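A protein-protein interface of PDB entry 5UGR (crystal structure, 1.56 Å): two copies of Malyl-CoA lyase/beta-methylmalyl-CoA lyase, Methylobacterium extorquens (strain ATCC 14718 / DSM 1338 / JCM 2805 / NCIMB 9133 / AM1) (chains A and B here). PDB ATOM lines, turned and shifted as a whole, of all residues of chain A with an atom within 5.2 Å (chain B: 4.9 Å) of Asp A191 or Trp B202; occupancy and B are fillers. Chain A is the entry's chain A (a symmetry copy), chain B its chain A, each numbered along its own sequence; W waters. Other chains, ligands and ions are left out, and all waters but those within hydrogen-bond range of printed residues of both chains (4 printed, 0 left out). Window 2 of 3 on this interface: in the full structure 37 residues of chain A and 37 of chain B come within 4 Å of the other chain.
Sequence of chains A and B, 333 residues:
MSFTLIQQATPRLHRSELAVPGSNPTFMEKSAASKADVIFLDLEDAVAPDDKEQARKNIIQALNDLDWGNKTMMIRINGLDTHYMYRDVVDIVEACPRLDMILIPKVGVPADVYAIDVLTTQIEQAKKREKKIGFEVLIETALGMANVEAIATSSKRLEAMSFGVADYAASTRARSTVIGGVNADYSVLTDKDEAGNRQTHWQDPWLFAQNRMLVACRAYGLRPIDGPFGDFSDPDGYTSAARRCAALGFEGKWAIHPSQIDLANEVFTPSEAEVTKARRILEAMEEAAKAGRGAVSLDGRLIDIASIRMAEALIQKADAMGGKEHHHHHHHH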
ATOM      1  N   VAL A 188     -10.038  29.914  -8.216  1.00  0.00           N
ATOM      2  CA  VAL A 188     -11.247  29.983  -9.015  1.00  0.00           C
ATOM      3  C   VAL A 188     -12.130  28.773  -8.789  1.00  0.00           C
ATOM      4  O   VAL A 188     -11.658  27.654  -8.578  1.00  0.00           O
ATOM      5  CB  VAL A 188     -11.010  30.211 -10.515  1.00  0.00           C
ATOM      6  CG1 VAL A 188     -10.243  31.520 -10.759  1.00  0.00           C
ATOM      7  CG2 VAL A 188     -10.343  29.005 -11.154  1.00  0.00           C
ATOM      8  N   LEU A 189     -13.432  29.054  -8.802  1.00  0.00           N
ATOM      9  CA  LEU A 189     -14.489  28.006  -8.661  1.00  0.00           C
ATOM     10  C   LEU A 189     -15.013  27.753 -10.055  1.00  0.00           C
ATOM     11  O   LEU A 189     -15.521  28.683 -10.688  1.00  0.00           O
ATOM     12  CB  LEU A 189     -15.599  28.486  -7.766  1.00  0.00           C
ATOM     13  CG  LEU A 189     -16.755  27.499  -7.486  1.00  0.00           C
ATOM     14  CD1 LEU A 189     -16.256  26.272  -6.786  1.00  0.00           C
ATOM     15  CD2 LEU A 189     -17.892  28.196  -6.716  1.00  0.00           C
ATOM     16  N   THR A 190     -14.806  26.565 -10.585  1.00  0.00           N
ATOM     17  CA  THR A 190     -15.194  26.297 -11.939  1.00  0.00           C
ATOM     18  C   THR A 190     -16.723  26.288 -12.110  1.00  0.00           C
ATOM     19  O   THR A 190     -17.478  26.086 -11.186  1.00  0.00           O
ATOM     20  CB  THR A 190     -14.576  24.991 -12.458  1.00  0.00           C
ATOM     21  OG1 THR A 190     -15.176  23.843 -11.834  1.00  0.00           O
ATOM     22  CG2 THR A 190     -13.035  25.010 -12.271  1.00  0.00           C
ATOM     23  N   ASP A 191     -17.152  26.547 -13.359  1.00  0.00           N
ATOM     24  CA  ASP A 191     -18.531  26.396 -13.711  1.00  0.00           C
ATOM     25  C   ASP A 191     -18.925  24.917 -13.638  1.00  0.00           C
ATOM     26  O   ASP A 191     -18.114  24.047 -13.918  1.00  0.00           O
ATOM     27  CB  ASP A 191     -18.751  26.930 -15.139  1.00  0.00           C
ATOM     28  CG  ASP A 191     -18.435  28.425 -15.287  1.00  0.00           C
ATOM     29  OD1 ASP A 191     -18.743  29.228 -14.375  1.00  0.00           O
ATOM     30  OD2 ASP A 191     -17.895  28.810 -16.339  1.00  0.00           O
ATOM     31  N   LYS A 192     -20.178  24.642 -13.263  1.00  0.00           N
ATOM     32  CA  LYS A 192     -20.652  23.242 -13.156  1.00  0.00           C
ATOM     33  C   LYS A 192     -20.389  22.488 -14.416  1.00  0.00           C
ATOM     34  O   LYS A 192     -20.711  22.980 -15.525  1.00  0.00           O
ATOM     35  CB  LYS A 192     -22.110  23.140 -12.796  1.00  0.00           C
ATOM     36  CG  LYS A 192     -22.438  23.629 -11.415  1.00  0.00           C
ATOM     37  CD  LYS A 192     -23.926  23.478 -11.009  1.00  0.00           C
ATOM     38  CE  LYS A 192     -24.087  23.843  -9.546  1.00  0.00           C
ATOM     39  NZ  LYS A 192     -25.456  23.507  -9.084  1.00  0.00           N
ATOM     40  N   ASP A 193     -19.821  21.292 -14.281  1.00  0.00           N
ATOM     41  CA  ASP A 193     -19.675  20.406 -15.421  1.00  0.00           C
ATOM     42  C   ASP A 193     -20.944  19.592 -15.611  1.00  0.00           C
ATOM     43  O   ASP A 193     -21.963  19.842 -14.962  1.00  0.00           O
ATOM     44  CB  ASP A 193     -18.405  19.542 -15.273  1.00  0.00           C
ATOM     45  CG  ASP A 193     -18.465  18.569 -14.107  1.00  0.00           C
ATOM     46  OD1 ASP A 193     -19.564  18.284 -13.588  1.00  0.00           O
ATOM     47  OD2 ASP A 193     -17.354  18.090 -13.741  1.00  0.00           O
ATOM     48  N   ASN A 197     -20.671  19.228 -10.999  1.00  0.00           N
ATOM     49  CA  ASN A 197     -19.520  19.460 -10.102  1.00  0.00           C
ATOM     50  C   ASN A 197     -18.783  20.739 -10.429  1.00  0.00           C
ATOM     51  O   ASN A 197     -18.658  21.139 -11.605  1.00  0.00           O
ATOM     52  CB  ASN A 197     -18.550  18.282 -10.186  1.00  0.00           C
ATOM     53  CG  ASN A 197     -19.160  16.981  -9.692  1.00  0.00           C
ATOM     54  OD1 ASN A 197     -20.133  16.970  -8.948  1.00  0.00           O
ATOM     55  ND2 ASN A 197     -18.571  15.866 -10.118  1.00  0.00           N
ATOM     56  N   ARG A 198     -18.224  21.315  -9.373  1.00  0.00           N
ATOM     57  CA  ARG A 198     -17.392  22.478  -9.448  1.00  0.00           C
ATOM     58  C   ARG A 198     -16.100  22.288  -8.701  1.00  0.00           C
ATOM     59  O   ARG A 198     -16.132  21.946  -7.507  1.00  0.00           O
ATOM     60  CB  ARG A 198     -18.127  23.700  -8.885  1.00  0.00           C
ATOM     61  CG  ARG A 198     -19.474  23.937  -9.454  1.00  0.00           C
ATOM     62  CD  ARG A 198     -20.170  25.124  -8.792  1.00  0.00           C
ATOM     63  NE  ARG A 198     -19.747  26.388  -9.355  1.00  0.00           N
ATOM     64  CZ  ARG A 198     -20.353  27.559  -9.111  1.00  0.00           C
ATOM     65  NH1 ARG A 198     -21.393  27.644  -8.285  1.00  0.00           N
ATOM     66  NH2 ARG A 198     -19.966  28.661  -9.781  1.00  0.00           N
ATOM     67  N   HIS A 201      -9.655  25.605  -8.213  1.00  0.00           N
ATOM     68  CA  HIS A 201      -8.293  25.621  -8.751  1.00  0.00           C
ATOM     69  C   HIS A 201      -7.530  26.833  -8.220  1.00  0.00           C
ATOM     70  O   HIS A 201      -7.926  27.989  -8.415  1.00  0.00           O
ATOM     71  CB  HIS A 201      -8.292  25.583 -10.264  1.00  0.00           C
ATOM     72  CG  HIS A 201      -8.805  24.279 -10.800  1.00  0.00           C
ATOM     73  ND1 HIS A 201      -9.164  24.113 -12.105  1.00  0.00           N
ATOM     74  CD2 HIS A 201      -8.953  23.067 -10.215  1.00  0.00           C
ATOM     75  CE1 HIS A 201      -9.562  22.874 -12.304  1.00  0.00           C
ATOM     76  NE2 HIS A 201      -9.435  22.215 -11.174  1.00  0.00           N
ATOM     77  N   GLN A 203      -4.808  29.685  -7.553  1.00  0.00           N
ATOM     78  CA  GLN A 203      -4.033  30.600  -8.378  1.00  0.00           C
ATOM     79  C   GLN A 203      -2.835  31.114  -7.605  1.00  0.00           C
ATOM     80  O   GLN A 203      -2.687  30.849  -6.406  1.00  0.00           O
ATOM     81  CB  GLN A 203      -4.909  31.778  -8.858  1.00  0.00           C
ATOM     82  CG  GLN A 203      -6.210  31.362  -9.501  1.00  0.00           C
ATOM     83  CD  GLN A 203      -6.079  30.566 -10.714  1.00  0.00           C
ATOM     84  OE1 GLN A 203      -5.399  30.952 -11.669  1.00  0.00           O
ATOM     85  NE2 GLN A 203      -6.771  29.337 -10.695  1.00  0.00           N
ATOM     86  N   VAL B 182     -15.808  33.164 -14.725  1.00  0.00           N
ATOM     87  CA  VAL B 182     -14.674  32.427 -15.233  1.00  0.00           C
ATOM     88  C   VAL B 182     -15.038  31.739 -16.591  1.00  0.00           C
ATOM     89  O   VAL B 182     -16.150  31.934 -17.147  1.00  0.00           O
ATOM     90  CB  VAL B 182     -14.116  31.498 -14.158  1.00  0.00           C
ATOM     91  CG1 VAL B 182     -13.553  32.340 -13.014  1.00  0.00           C
ATOM     92  CG2 VAL B 182     -15.181  30.543 -13.697  1.00  0.00           C
ATOM     93  N   ASN B 183     -14.081  31.025 -17.146  1.00  0.00           N
ATOM     94  CA  ASN B 183     -14.218  30.534 -18.510  1.00  0.00           C
ATOM     95  C   ASN B 183     -13.460  29.235 -18.686  1.00  0.00           C
ATOM     96  O   ASN B 183     -12.225  29.215 -18.461  1.00  0.00           O
ATOM     97  CB  ASN B 183     -13.644  31.622 -19.440  1.00  0.00           C
ATOM     98  CG  ASN B 183     -13.913  31.397 -20.909  1.00  0.00           C
ATOM     99  OD1 ASN B 183     -14.073  32.385 -21.713  1.00  0.00           O
ATOM    100  ND2 ASN B 183     -14.011  30.199 -21.295  1.00  0.00           N
ATOM    101  N   ALA B 184     -14.139  28.150 -19.004  1.00  0.00           N
ATOM    102  CA  ALA B 184     -13.469  26.855 -19.199  1.00  0.00           C
ATOM    103  C   ALA B 184     -12.297  26.889 -20.190  1.00  0.00           C
ATOM    104  O   ALA B 184     -11.401  26.070 -20.097  1.00  0.00           O
ATOM    105  CB  ALA B 184     -14.464  25.825 -19.690  1.00  0.00           C
ATOM    106  N   TYR B 186     -10.286  29.479 -20.511  1.00  0.00           N
ATOM    107  CA  TYR B 186      -9.139  30.218 -19.950  1.00  0.00           C
ATOM    108  C   TYR B 186      -8.544  29.273 -18.889  1.00  0.00           C
ATOM    109  O   TYR B 186      -8.824  29.340 -17.673  1.00  0.00           O
ATOM    110  CB  TYR B 186      -9.524  31.583 -19.388  1.00  0.00           C
ATOM    111  CG  TYR B 186      -8.293  32.439 -19.210  1.00  0.00           C
ATOM    112  CD1 TYR B 186      -7.527  32.808 -20.285  1.00  0.00           C
ATOM    113  CD2 TYR B 186      -7.829  32.814 -17.952  1.00  0.00           C
ATOM    114  CE1 TYR B 186      -6.344  33.503 -20.169  1.00  0.00           C
ATOM    115  CE2 TYR B 186      -6.646  33.503 -17.811  1.00  0.00           C
ATOM    116  CZ  TYR B 186      -5.896  33.871 -18.918  1.00  0.00           C
ATOM    117  OH  TYR B 186      -4.729  34.590 -18.806  1.00  0.00           O
ATOM    118  N   SER B 187      -7.731  28.333 -19.414  1.00  0.00           N
ATOM    119  CA  SER B 187      -7.284  27.158 -18.682  1.00  0.00           C
ATOM    120  C   SER B 187      -6.037  26.652 -19.342  1.00  0.00           C
ATOM    121  O   SER B 187      -5.772  26.941 -20.514  1.00  0.00           O
ATOM    122  CB  SER B 187      -8.397  26.080 -18.686  1.00  0.00           C
ATOM    123  OG  SER B 187      -8.730  25.635 -19.986  1.00  0.00           O
ATOM    124  N   THR B 200      -7.078  19.685 -16.873  1.00  0.00           N
ATOM    125  CA  THR B 200      -7.398  21.056 -17.280  1.00  0.00           C
ATOM    126  C   THR B 200      -7.518  21.866 -15.988  1.00  0.00           C
ATOM    127  O   THR B 200      -8.470  21.678 -15.208  1.00  0.00           O
ATOM    128  CB  THR B 200      -8.667  21.097 -18.135  1.00  0.00           C
ATOM    129  OG1 THR B 200      -8.432  20.372 -19.361  1.00  0.00           O
ATOM    130  CG2 THR B 200      -9.087  22.529 -18.438  1.00  0.00           C
ATOM    131  N   HIS B 201      -6.599  22.810 -15.821  1.00  0.00           N
ATOM    132  CA  HIS B 201      -6.570  23.685 -14.648  1.00  0.00           C
ATOM    133  C   HIS B 201      -6.969  25.107 -15.038  1.00  0.00           C
ATOM    134  O   HIS B 201      -6.340  25.750 -15.888  1.00  0.00           O
ATOM    135  CB  HIS B 201      -5.219  23.657 -13.965  1.00  0.00           C
ATOM    136  CG  HIS B 201      -4.924  22.323 -13.345  1.00  0.00           C
ATOM    137  ND1 HIS B 201      -3.675  21.966 -12.929  1.00  0.00           N
ATOM    138  CD2 HIS B 201      -5.737  21.291 -13.011  1.00  0.00           C
ATOM    139  CE1 HIS B 201      -3.705  20.756 -12.415  1.00  0.00           C
ATOM    140  NE2 HIS B 201      -4.947  20.326 -12.443  1.00  0.00           N
ATOM    141  N   TRP B 202      -8.072  25.560 -14.468  1.00  0.00           N
ATOM    142  CA  TRP B 202      -8.633  26.845 -14.842  1.00  0.00           C
ATOM    143  C   TRP B 202      -7.809  27.981 -14.279  1.00  0.00           C
ATOM    144  O   TRP B 202      -7.234  27.869 -13.181  1.00  0.00           O
ATOM    145  CB  TRP B 202     -10.099  26.971 -14.437  1.00  0.00           C
ATOM    146  CG  TRP B 202     -11.053  26.016 -15.099  1.00  0.00           C
ATOM    147  CD1 TRP B 202     -10.853  24.699 -15.391  1.00  0.00           C
ATOM    148  CD2 TRP B 202     -12.414  26.297 -15.425  1.00  0.00           C
ATOM    149  NE1 TRP B 202     -12.015  24.141 -15.870  1.00  0.00           N
ATOM    150  CE2 TRP B 202     -12.996  25.099 -15.898  1.00  0.00           C
ATOM    151  CE3 TRP B 202     -13.201  27.437 -15.346  1.00  0.00           C
ATOM    152  CZ2 TRP B 202     -14.324  25.040 -16.321  1.00  0.00           C
ATOM    153  CZ3 TRP B 202     -14.529  27.363 -15.760  1.00  0.00           C
ATOM    154  CH2 TRP B 202     -15.064  26.183 -16.240  1.00  0.00           C
ATOM    155  N   GLN B 203      -7.697  29.038 -15.061  1.00  0.00           N
ATOM    156  CA  GLN B 203      -6.963  30.238 -14.684  1.00  0.00           C
ATOM    157  C   GLN B 203      -7.920  31.395 -14.479  1.00  0.00           C
ATOM    158  O   GLN B 203      -9.123  31.284 -14.748  1.00  0.00           O
ATOM    159  CB  GLN B 203      -5.910  30.593 -15.756  1.00  0.00           C
ATOM    160  CG  GLN B 203      -5.007  29.446 -16.143  1.00  0.00           C
ATOM    161  CD  GLN B 203      -4.180  28.913 -15.069  1.00  0.00           C
ATOM    162  OE1 GLN B 203      -3.444  29.642 -14.400  1.00  0.00           O
ATOM    163  NE2 GLN B 203      -4.305  27.525 -14.858  1.00  0.00           N
ATOM    164  N   ASP B 204      -7.377  32.526 -14.026  1.00  0.00           N
ATOM    165  CA  ASP B 204      -8.203  33.690 -13.670  1.00  0.00           C
ATOM    166  C   ASP B 204      -8.101  34.713 -14.792  1.00  0.00           C
ATOM    167  O   ASP B 204      -7.096  35.400 -14.903  1.00  0.00           O
ATOM    168  CB  ASP B 204      -7.706  34.264 -12.350  1.00  0.00           C
ATOM    169  CG  ASP B 204      -8.492  35.458 -11.862  1.00  0.00           C
ATOM    170  OD1 ASP B 204      -9.340  35.984 -12.594  1.00  0.00           O
ATOM    171  OD2 ASP B 204      -8.212  35.869 -10.711  1.00  0.00           O
HETATM  172  O   HOH W   1     -19.064  31.077 -17.383  1.00  0.00           O
HETATM  173  O   HOH W   2     -17.058  28.068 -18.724  1.00  0.00           O
HETATM  174  O   HOH W   3     -18.502  31.897 -14.579  1.00  0.00           O
HETATM  175  O   HOH W   4      -4.470  32.626 -13.256  1.00  0.00           O
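The backbone NH of Trp B202 sits at hydrogen-bond distance from a ring nitrogen (ND1) of His A201 (3.0 Å). NE2 of Gln A203 is in hydrogen-bond range of O of Trp B202 (2.9 Å). OE1 of Gln A203 is in hydrogen-bond range of N of Asp B204.
The backbone NH (N) of Gln B203 is in hydrogen-bond range of the backbone carbonyl oxygen (O) of Tyr B186 (2.9 Å). The backbone carbonyl oxygen (O) of His B201 is in hydrogen-bond range of the side-chain amide nitrogen (NE2) of Gln B203 (2.9 Å). N of Val A188 is in hydrogen-bond range of O of His A201. The backbone carbonyl oxygen (O) of Thr A190 lies within hydrogen-bond range of the guanidinium group (NE) of Arg A198, 2.9 Å away. NE2 of Gln A203 lies within hydrogen-bond range of O of His A201.
Among the printed residues, merely in contact across the chains: His A201 with Thr B200 (3.3 Å), Thr A190 with Trp B202 (3.5 Å), Gln A203 with Gln B203 (3.5 Å), Leu A189 with Val B182 (3.6 Å), Asp A191 with Trp B202 (3.6 Å), His A201 with His B201 (3.7 Å), Asp A191 with Val B182 (3.7 Å) and Val A188 with Trp B202 (3.9 Å).
Printed residues of chain A within 4 Å of Trp B202: Val A188 (3.9 Å), Thr A190 (3.5 Å), Asp A191 (3.6 Å), His A201 (3.0 Å) and Gln A203 (2.9 Å). Printed residues of chain B within 4 Å of Val A188: Trp B202. Of the printed residues of chain A, Val B182 touches Leu A189 (3.6 Å) and Asp A191 (3.7 Å). Of the printed residues of chain B, His A201 touches Thr B200 (3.3 Å), His B201 (3.7 Å) and Trp B202 (3.0 Å). Of the printed residues of chain A, Gln B203 touches Gln A203. Of the printed residues of chain A, His B201 touches His A201 (3.7 Å). Asp A193 touches none of the printed residues of chain B. Arg A198 touches none of the printed residues of chain B. The nearest residue of chain B that does not touch Asp A191 is Asn B183 (4.5 Å).
Of the 10 printed residues of chain B, 6 touch a printed residue of chain A. Printed residues of chain B that touch a printed residue of chain A: Val B182, Thr B200, His B201, Trp B202, Gln B203 and Asp B204. Of the 10 printed residues of chain A, 6 touch a printed residue of chain B. Among the printed residues, 11 pairs touch across the chains.
His A201 touches its own counterpart, His B201. Gln A203 touches its own counterpart, Gln B203. Of the 11 pairs that touch across the chains among the printed residues, 2 have their exchanged pair printed and touching as well.
Water W4 lies within hydrogen-bond range of the side-chain amide oxygen (OE1) of Gln A203, the backbone NH (N) of Asp B204 and the side-chain amide oxygen (OE1) of Gln B203. Water W2 bridges OD2 of Asp A191 (2.6 Å) and N of Ala B184 (2.9 Å). Water W3 bridges the side-chain carboxylate (OD1) of Asp A191 and the backbone NH (N) of Val B182. Water W1 lies within hydrogen-bond range of OD2 of Asp A191 (2.8 Å) and O of Val B182 (3.0 Å).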
